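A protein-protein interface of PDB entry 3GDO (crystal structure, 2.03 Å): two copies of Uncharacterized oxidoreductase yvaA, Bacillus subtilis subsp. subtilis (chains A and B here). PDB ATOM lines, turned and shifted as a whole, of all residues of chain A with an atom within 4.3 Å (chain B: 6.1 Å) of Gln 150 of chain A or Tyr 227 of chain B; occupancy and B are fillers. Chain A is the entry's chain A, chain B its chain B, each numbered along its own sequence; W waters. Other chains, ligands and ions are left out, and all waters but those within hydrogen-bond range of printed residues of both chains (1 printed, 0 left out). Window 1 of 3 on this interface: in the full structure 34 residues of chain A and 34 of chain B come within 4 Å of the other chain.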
ATOM      1  N   THR A 148     -31.584  -1.208   4.826  1.00  0.00           N
ATOM      2  CA  THR A 148     -30.541  -2.192   5.132  1.00  0.00           C
ATOM      3  C   THR A 148     -30.063  -2.918   3.873  1.00  0.00           C
ATOM      4  O   THR A 148     -30.869  -3.488   3.127  1.00  0.00           O
ATOM      5  CB  THR A 148     -31.045  -3.242   6.138  1.00  0.00           C
ATOM      6  OG1 THR A 148     -31.518  -2.580   7.316  1.00  0.00           O
ATOM      7  CG2 THR A 148     -29.937  -4.238   6.509  1.00  0.00           C
ATOM      8  N   TYR A 149     -28.754  -2.943   3.670  1.00  0.00           N
ATOM      9  CA  TYR A 149     -28.166  -3.597   2.500  1.00  0.00           C
ATOM     10  C   TYR A 149     -27.011  -4.477   2.970  1.00  0.00           C
ATOM     11  O   TYR A 149     -25.900  -3.969   3.280  1.00  0.00           O
ATOM     12  CB  TYR A 149     -27.739  -2.513   1.527  1.00  0.00           C
ATOM     13  CG  TYR A 149     -27.060  -2.943   0.262  1.00  0.00           C
ATOM     14  CD1 TYR A 149     -27.807  -3.243  -0.880  1.00  0.00           C
ATOM     15  CD2 TYR A 149     -25.676  -3.043   0.190  1.00  0.00           C
ATOM     16  CE1 TYR A 149     -27.184  -3.627  -2.036  1.00  0.00           C
ATOM     17  CE2 TYR A 149     -25.045  -3.418  -0.961  1.00  0.00           C
ATOM     18  CZ  TYR A 149     -25.820  -3.697  -2.096  1.00  0.00           C
ATOM     19  OH  TYR A 149     -25.230  -4.083  -3.276  1.00  0.00           O
ATOM     20  N   GLN A 150     -27.261  -5.796   3.020  1.00  0.00           N
ATOM     21  CA  GLN A 150     -26.272  -6.744   3.533  1.00  0.00           C
ATOM     22  C   GLN A 150     -25.760  -7.681   2.478  1.00  0.00           C
ATOM     23  O   GLN A 150     -26.555  -8.344   1.837  1.00  0.00           O
ATOM     24  CB  GLN A 150     -26.875  -7.613   4.633  1.00  0.00           C
ATOM     25  CG  GLN A 150     -27.493  -6.777   5.667  1.00  0.00           C
ATOM     26  CD  GLN A 150     -28.094  -7.543   6.802  1.00  0.00           C
ATOM     27  OE1 GLN A 150     -28.704  -8.617   6.633  1.00  0.00           O
ATOM     28  NE2 GLN A 150     -27.980  -6.955   7.987  1.00  0.00           N
ATOM     29  N   VAL A 151     -24.441  -7.746   2.329  1.00  0.00           N
ATOM     30  CA  VAL A 151     -23.836  -8.492   1.222  1.00  0.00           C
ATOM     31  C   VAL A 151     -22.749  -9.394   1.746  1.00  0.00           C
ATOM     32  O   VAL A 151     -21.853  -8.933   2.468  1.00  0.00           O
ATOM     33  CB  VAL A 151     -23.191  -7.588   0.141  1.00  0.00           C
ATOM     34  CG1 VAL A 151     -22.654  -8.474  -1.005  1.00  0.00           C
ATOM     35  CG2 VAL A 151     -24.209  -6.567  -0.347  1.00  0.00           C
ATOM     36  N   ILE A 225     -23.903  -3.450   5.164  1.00  0.00           N
ATOM     37  CA  ILE A 225     -23.031  -4.388   5.852  1.00  0.00           C
ATOM     38  C   ILE A 225     -22.401  -5.304   4.808  1.00  0.00           C
ATOM     39  O   ILE A 225     -23.142  -6.041   4.092  1.00  0.00           O
ATOM     40  CB  ILE A 225     -23.858  -5.280   6.831  1.00  0.00           C
ATOM     41  CG1 ILE A 225     -24.778  -4.455   7.732  1.00  0.00           C
ATOM     42  CG2 ILE A 225     -22.957  -6.177   7.673  1.00  0.00           C
ATOM     43  CD1 ILE A 225     -24.061  -3.410   8.526  1.00  0.00           C
ATOM     44  N   ARG A 238     -26.280 -14.168  -0.670  1.00  0.00           N
ATOM     45  CA  ARG A 238     -25.304 -13.164  -1.069  1.00  0.00           C
ATOM     46  C   ARG A 238     -25.916 -11.785  -0.775  1.00  0.00           C
ATOM     47  O   ARG A 238     -25.209 -10.894  -0.276  1.00  0.00           O
ATOM     48  CB  ARG A 238     -24.867 -13.369  -2.534  1.00  0.00           C
ATOM     49  CG  ARG A 238     -23.929 -12.321  -3.104  1.00  0.00           C
ATOM     50  CD  ARG A 238     -23.330 -12.718  -4.485  1.00  0.00           C
ATOM     51  NE  ARG A 238     -22.582 -11.601  -5.042  1.00  0.00           N
ATOM     52  CZ  ARG A 238     -21.249 -11.463  -4.985  1.00  0.00           C
ATOM     53  NH1 ARG A 238     -20.499 -12.369  -4.390  1.00  0.00           N
ATOM     54  NH2 ARG A 238     -20.670 -10.397  -5.506  1.00  0.00           N
ATOM     55  N   TYR A 239     -27.221 -11.628  -1.011  1.00  0.00           N
ATOM     56  CA  TYR A 239     -27.882 -10.322  -0.848  1.00  0.00           C
ATOM     57  C   TYR A 239     -29.102 -10.420   0.059  1.00  0.00           C
ATOM     58  O   TYR A 239     -29.968 -11.303  -0.124  1.00  0.00           O
ATOM     59  CB  TYR A 239     -28.332  -9.683  -2.198  1.00  0.00           C
ATOM     60  CG  TYR A 239     -27.191  -9.336  -3.121  1.00  0.00           C
ATOM     61  CD1 TYR A 239     -26.515  -8.118  -2.993  1.00  0.00           C
ATOM     62  CD2 TYR A 239     -26.791 -10.215  -4.145  1.00  0.00           C
ATOM     63  CE1 TYR A 239     -25.417  -7.825  -3.788  1.00  0.00           C
ATOM     64  CE2 TYR A 239     -25.718  -9.914  -4.971  1.00  0.00           C
ATOM     65  CZ  TYR A 239     -25.047  -8.710  -4.785  1.00  0.00           C
ATOM     66  OH  TYR A 239     -23.983  -8.411  -5.584  1.00  0.00           O
ATOM     67  N   GLN A 240     -29.181  -9.501   1.022  1.00  0.00           N
ATOM     68  CA  GLN A 240     -30.406  -9.273   1.774  1.00  0.00           C
ATOM     69  C   GLN A 240     -30.587  -7.766   1.766  1.00  0.00           C
ATOM     70  O   GLN A 240     -29.706  -7.021   2.237  1.00  0.00           O
ATOM     71  CB  GLN A 240     -30.267  -9.834   3.209  1.00  0.00           C
ATOM     72  CG  GLN A 240     -29.813 -11.307   3.225  1.00  0.00           C
ATOM     73  CD  GLN A 240     -29.492 -11.853   4.625  1.00  0.00           C
ATOM     74  OE1 GLN A 240     -30.383 -12.001   5.435  1.00  0.00           O
ATOM     75  NE2 GLN A 240     -28.209 -12.176   4.887  1.00  0.00           N
ATOM     76  N   GLN B 150     -23.984 -16.207  13.385  1.00  0.00           N
ATOM     77  CA  GLN B 150     -24.699 -14.979  12.965  1.00  0.00           C
ATOM     78  C   GLN B 150     -26.162 -15.204  13.144  1.00  0.00           C
ATOM     79  O   GLN B 150     -26.720 -16.179  12.603  1.00  0.00           O
ATOM     80  CB  GLN B 150     -24.441 -14.644  11.488  1.00  0.00           C
ATOM     81  CG  GLN B 150     -23.032 -14.187  11.215  1.00  0.00           C
ATOM     82  CD  GLN B 150     -22.763 -13.944   9.719  1.00  0.00           C
ATOM     83  OE1 GLN B 150     -23.467 -14.483   8.845  1.00  0.00           O
ATOM     84  NE2 GLN B 150     -21.716 -13.153   9.425  1.00  0.00           N
ATOM     85  N   VAL B 151     -26.782 -14.331  13.924  1.00  0.00           N
ATOM     86  CA  VAL B 151     -28.196 -14.528  14.284  1.00  0.00           C
ATOM     87  C   VAL B 151     -28.944 -13.254  13.958  1.00  0.00           C
ATOM     88  O   VAL B 151     -28.483 -12.141  14.320  1.00  0.00           O
ATOM     89  CB  VAL B 151     -28.378 -14.893  15.813  1.00  0.00           C
ATOM     90  CG1 VAL B 151     -29.801 -15.264  16.093  1.00  0.00           C
ATOM     91  CG2 VAL B 151     -27.447 -16.053  16.176  1.00  0.00           C
ATOM     92  N   SER B 152     -30.056 -13.379  13.248  1.00  0.00           N
ATOM     93  CA  SER B 152     -30.882 -12.165  13.040  1.00  0.00           C
ATOM     94  C   SER B 152     -32.262 -12.270  13.602  1.00  0.00           C
ATOM     95  O   SER B 152     -32.856 -13.350  13.655  1.00  0.00           O
ATOM     96  CB  SER B 152     -30.925 -11.712  11.579  1.00  0.00           C
ATOM     97  OG  SER B 152     -31.783 -12.502  10.817  1.00  0.00           O
ATOM     98  N   TYR B 153     -32.801 -11.150  14.048  1.00  0.00           N
ATOM     99  CA  TYR B 153     -34.080 -11.183  14.763  1.00  0.00           C
ATOM    100  C   TYR B 153     -34.847  -9.934  14.375  1.00  0.00           C
ATOM    101  O   TYR B 153     -34.785  -8.915  15.053  1.00  0.00           O
ATOM    102  CB  TYR B 153     -33.811 -11.169  16.267  1.00  0.00           C
ATOM    103  CG  TYR B 153     -34.949 -11.632  17.163  1.00  0.00           C
ATOM    104  CD1 TYR B 153     -34.680 -12.046  18.485  1.00  0.00           C
ATOM    105  CD2 TYR B 153     -36.279 -11.693  16.709  1.00  0.00           C
ATOM    106  CE1 TYR B 153     -35.702 -12.462  19.312  1.00  0.00           C
ATOM    107  CE2 TYR B 153     -37.307 -12.139  17.530  1.00  0.00           C
ATOM    108  CZ  TYR B 153     -37.005 -12.499  18.840  1.00  0.00           C
ATOM    109  OH  TYR B 153     -37.986 -12.904  19.691  1.00  0.00           O
ATOM    110  N   ASN B 154     -35.563 -10.029  13.266  1.00  0.00           N
ATOM    111  CA  ASN B 154     -36.076  -8.859  12.596  1.00  0.00           C
ATOM    112  C   ASN B 154     -37.564  -8.806  12.778  1.00  0.00           C
ATOM    113  O   ASN B 154     -38.182  -9.810  13.089  1.00  0.00           O
ATOM    114  CB  ASN B 154     -35.793  -8.950  11.100  1.00  0.00           C
ATOM    115  CG  ASN B 154     -34.348  -8.868  10.765  1.00  0.00           C
ATOM    116  OD1 ASN B 154     -33.624  -7.950  11.179  1.00  0.00           O
ATOM    117  ND2 ASN B 154     -33.911  -9.796   9.953  1.00  0.00           N
ATOM    118  N   ILE B 182     -31.150 -13.475  22.104  1.00  0.00           N
ATOM    119  CA  ILE B 182     -30.136 -14.093  21.244  1.00  0.00           C
ATOM    120  C   ILE B 182     -28.726 -13.884  21.806  1.00  0.00           C
ATOM    121  O   ILE B 182     -27.818 -14.671  21.542  1.00  0.00           O
ATOM    122  CB  ILE B 182     -30.310 -13.655  19.740  1.00  0.00           C
ATOM    123  CG1 ILE B 182     -30.232 -12.128  19.570  1.00  0.00           C
ATOM    124  CG2 ILE B 182     -31.671 -14.150  19.208  1.00  0.00           C
ATOM    125  CD1 ILE B 182     -30.107 -11.699  18.042  1.00  0.00           C
ATOM    126  N   TYR B 212     -33.302  -0.836  16.044  1.00  0.00           N
ATOM    127  CA  TYR B 212     -32.263  -1.446  15.251  1.00  0.00           C
ATOM    128  C   TYR B 212     -31.018  -1.692  16.103  1.00  0.00           C
ATOM    129  O   TYR B 212     -30.544  -0.796  16.827  1.00  0.00           O
ATOM    130  CB  TYR B 212     -31.925  -0.523  14.060  1.00  0.00           C
ATOM    131  CG  TYR B 212     -30.776  -1.000  13.221  1.00  0.00           C
ATOM    132  CD1 TYR B 212     -30.994  -1.646  11.999  1.00  0.00           C
ATOM    133  CD2 TYR B 212     -29.458  -0.835  13.658  1.00  0.00           C
ATOM    134  CE1 TYR B 212     -29.916  -2.108  11.219  1.00  0.00           C
ATOM    135  CE2 TYR B 212     -28.392  -1.304  12.940  1.00  0.00           C
ATOM    136  CZ  TYR B 212     -28.625  -1.955  11.715  1.00  0.00           C
ATOM    137  OH  TYR B 212     -27.551  -2.357  10.986  1.00  0.00           O
ATOM    138  N   PHE B 213     -30.456  -2.890  15.990  1.00  0.00           N
ATOM    139  CA  PHE B 213     -29.166  -3.162  16.614  1.00  0.00           C
ATOM    140  C   PHE B 213     -28.370  -4.121  15.755  1.00  0.00           C
ATOM    141  O   PHE B 213     -28.917  -5.062  15.115  1.00  0.00           O
ATOM    142  CB  PHE B 213     -29.336  -3.723  18.058  1.00  0.00           C
ATOM    143  CG  PHE B 213     -30.040  -5.051  18.107  1.00  0.00           C
ATOM    144  CD1 PHE B 213     -29.333  -6.247  17.896  1.00  0.00           C
ATOM    145  CD2 PHE B 213     -31.401  -5.119  18.326  1.00  0.00           C
ATOM    146  CE1 PHE B 213     -29.992  -7.466  17.899  1.00  0.00           C
ATOM    147  CE2 PHE B 213     -32.064  -6.325  18.307  1.00  0.00           C
ATOM    148  CZ  PHE B 213     -31.351  -7.512  18.122  1.00  0.00           C
ATOM    149  N   HIS B 214     -27.075  -3.894  15.777  1.00  0.00           N
ATOM    150  CA  HIS B 214     -26.121  -4.781  15.156  1.00  0.00           C
ATOM    151  C   HIS B 214     -24.926  -4.940  16.123  1.00  0.00           C
ATOM    152  O   HIS B 214     -24.190  -3.985  16.370  1.00  0.00           O
ATOM    153  CB  HIS B 214     -25.631  -4.161  13.834  1.00  0.00           C
ATOM    154  CG  HIS B 214     -24.884  -5.134  13.001  1.00  0.00           C
ATOM    155  ND1 HIS B 214     -23.566  -5.481  13.262  1.00  0.00           N
ATOM    156  CD2 HIS B 214     -25.298  -5.929  11.980  1.00  0.00           C
ATOM    157  CE1 HIS B 214     -23.191  -6.411  12.394  1.00  0.00           C
ATOM    158  NE2 HIS B 214     -24.225  -6.709  11.617  1.00  0.00           N
ATOM    159  N   LEU B 215     -24.742  -6.115  16.691  1.00  0.00           N
ATOM    160  CA  LEU B 215     -23.656  -6.306  17.654  1.00  0.00           C
ATOM    161  C   LEU B 215     -22.648  -7.321  17.150  1.00  0.00           C
ATOM    162  O   LEU B 215     -23.031  -8.350  16.592  1.00  0.00           O
ATOM    163  CB  LEU B 215     -24.221  -6.840  18.989  1.00  0.00           C
ATOM    164  CG  LEU B 215     -24.734  -5.913  20.087  1.00  0.00           C
ATOM    165  CD1 LEU B 215     -25.896  -5.036  19.589  1.00  0.00           C
ATOM    166  CD2 LEU B 215     -25.198  -6.795  21.246  1.00  0.00           C
ATOM    167  N   ILE B 225     -22.260 -12.522  15.604  1.00  0.00           N
ATOM    168  CA  ILE B 225     -22.833 -11.291  15.056  1.00  0.00           C
ATOM    169  C   ILE B 225     -24.324 -11.365  15.349  1.00  0.00           C
ATOM    170  O   ILE B 225     -24.967 -12.321  14.911  1.00  0.00           O
ATOM    171  CB  ILE B 225     -22.649 -11.180  13.508  1.00  0.00           C
ATOM    172  CG1 ILE B 225     -21.186 -11.308  13.034  1.00  0.00           C
ATOM    173  CG2 ILE B 225     -23.413  -9.937  12.939  1.00  0.00           C
ATOM    174  CD1 ILE B 225     -20.217 -10.367  13.601  1.00  0.00           C
ATOM    175  N   LEU B 226     -24.878 -10.377  16.060  1.00  0.00           N
ATOM    176  CA  LEU B 226     -26.289 -10.449  16.483  1.00  0.00           C
ATOM    177  C   LEU B 226     -26.952  -9.162  16.082  1.00  0.00           C
ATOM    178  O   LEU B 226     -26.463  -8.070  16.427  1.00  0.00           O
ATOM    179  CB  LEU B 226     -26.426 -10.624  17.999  1.00  0.00           C
ATOM    180  CG  LEU B 226     -25.648 -11.778  18.615  1.00  0.00           C
ATOM    181  CD1 LEU B 226     -25.565 -11.583  20.143  1.00  0.00           C
ATOM    182  CD2 LEU B 226     -26.309 -13.100  18.265  1.00  0.00           C
ATOM    183  N   TYR B 227     -28.025  -9.283  15.296  1.00  0.00           N
ATOM    184  CA  TYR B 227     -28.599  -8.096  14.691  1.00  0.00           C
ATOM    185  C   TYR B 227     -30.079  -8.242  14.488  1.00  0.00           C
ATOM    186  O   TYR B 227     -30.617  -9.363  14.459  1.00  0.00           O
ATOM    187  CB  TYR B 227     -27.871  -7.743  13.384  1.00  0.00           C
ATOM    188  CG  TYR B 227     -28.054  -8.721  12.259  1.00  0.00           C
ATOM    189  CD1 TYR B 227     -29.099  -8.553  11.338  1.00  0.00           C
ATOM    190  CD2 TYR B 227     -27.176  -9.831  12.105  1.00  0.00           C
ATOM    191  CE1 TYR B 227     -29.270  -9.435  10.300  1.00  0.00           C
ATOM    192  CE2 TYR B 227     -27.350 -10.742  11.043  1.00  0.00           C
ATOM    193  CZ  TYR B 227     -28.398 -10.525  10.142  1.00  0.00           C
ATOM    194  OH  TYR B 227     -28.615 -11.378   9.079  1.00  0.00           O
ATOM    195  N   GLY B 228     -30.733  -7.109  14.328  1.00  0.00           N
ATOM    196  CA  GLY B 228     -32.184  -7.056  14.302  1.00  0.00           C
ATOM    197  C   GLY B 228     -32.611  -5.702  13.789  1.00  0.00           C
ATOM    198  O   GLY B 228     -32.081  -4.670  14.241  1.00  0.00           O
ATOM    199  N   GLY B 229     -33.523  -5.699  12.819  1.00  0.00           N
ATOM    200  CA  GLY B 229     -34.218  -4.442  12.436  1.00  0.00           C
ATOM    201  C   GLY B 229     -35.730  -4.481  12.534  1.00  0.00           C
ATOM    202  O   GLY B 229     -36.341  -5.558  12.723  1.00  0.00           O
ATOM    203  N   PRO B 237     -32.187 -15.919   6.870  1.00  0.00           N
ATOM    204  CA  PRO B 237     -32.058 -16.910   7.932  1.00  0.00           C
ATOM    205  C   PRO B 237     -31.926 -16.284   9.348  1.00  0.00           C
ATOM    206  O   PRO B 237     -31.316 -15.193   9.530  1.00  0.00           O
ATOM    207  CB  PRO B 237     -30.754 -17.597   7.606  1.00  0.00           C
ATOM    208  CG  PRO B 237     -30.309 -17.099   6.272  1.00  0.00           C
ATOM    209  CD  PRO B 237     -31.088 -15.949   5.893  1.00  0.00           C
ATOM    210  N   GLN B 240     -27.124 -18.511  10.938  1.00  0.00           N
ATOM    211  CA  GLN B 240     -26.111 -18.958  10.013  1.00  0.00           C
ATOM    212  C   GLN B 240     -24.881 -19.239  10.836  1.00  0.00           C
ATOM    213  O   GLN B 240     -24.236 -18.304  11.414  1.00  0.00           O
ATOM    214  CB  GLN B 240     -25.801 -17.883   8.942  1.00  0.00           C
ATOM    215  CG  GLN B 240     -27.017 -17.467   8.103  1.00  0.00           C
ATOM    216  CD  GLN B 240     -26.766 -16.233   7.216  1.00  0.00           C
ATOM    217  OE1 GLN B 240     -26.014 -16.283   6.252  1.00  0.00           O
ATOM    218  NE2 GLN B 240     -27.438 -15.129   7.540  1.00  0.00           N
HETATM  219  O   HOH W   1     -30.402 -13.094   8.064  1.00  0.00           O
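Of the 17 printed residues of chain B, 1 touches a printed residue of chain A.
Hydrophobic or aromatic side chains of chain B that line the printed part of chain A: Tyr 227.
Among the printed residues, 1 pair touches across the chains.
Among the printed residues, no Asp or Glu carboxylate lies within 4 Å of a Lys or Arg side-chain nitrogen of the other chain.
Positions printed for both chains: 150, 151, 225 and 240.
The backbone carbonyl oxygen (O) of Gln 240 of chain A lies within hydrogen-bond range of the backbone NH (N) of Gln 150 of chain A (2.8 Å).
The backbone carbonyl oxygen (O) of Val 151 of chain B is in hydrogen-bond range of the backbone NH (N) of Tyr 227 of chain B.
O of Tyr 227 of chain B sits at hydrogen-bond distance from N of Tyr 153 of chain B, 2.9 Å away.
Water W1 lies within hydrogen-bond range of the side-chain hydroxyl (OH) of Tyr 227 of chain B (2.7 Å), the backbone carbonyl oxygen (O) of Pro 237 of chain B (2.7 Å), the side-chain amide oxygen (OE1) of Gln 240 of chain A (2.8 Å) and the side-chain hydroxyl (OG) of Ser 152 of chain B (3.1 Å).
Gln 150 of chain A touches just one residue of chain B: Tyr 227 (3.6 Å).
Of the printed residues of chain A, Tyr 227 of chain B touches Gln 150.
His 214 of chain B touches none of the printed residues of chain A.
Thr 148 of chain A touches none of the printed residues of chain B.
Tyr 227 of chain B touches Gln 150 of chain A.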
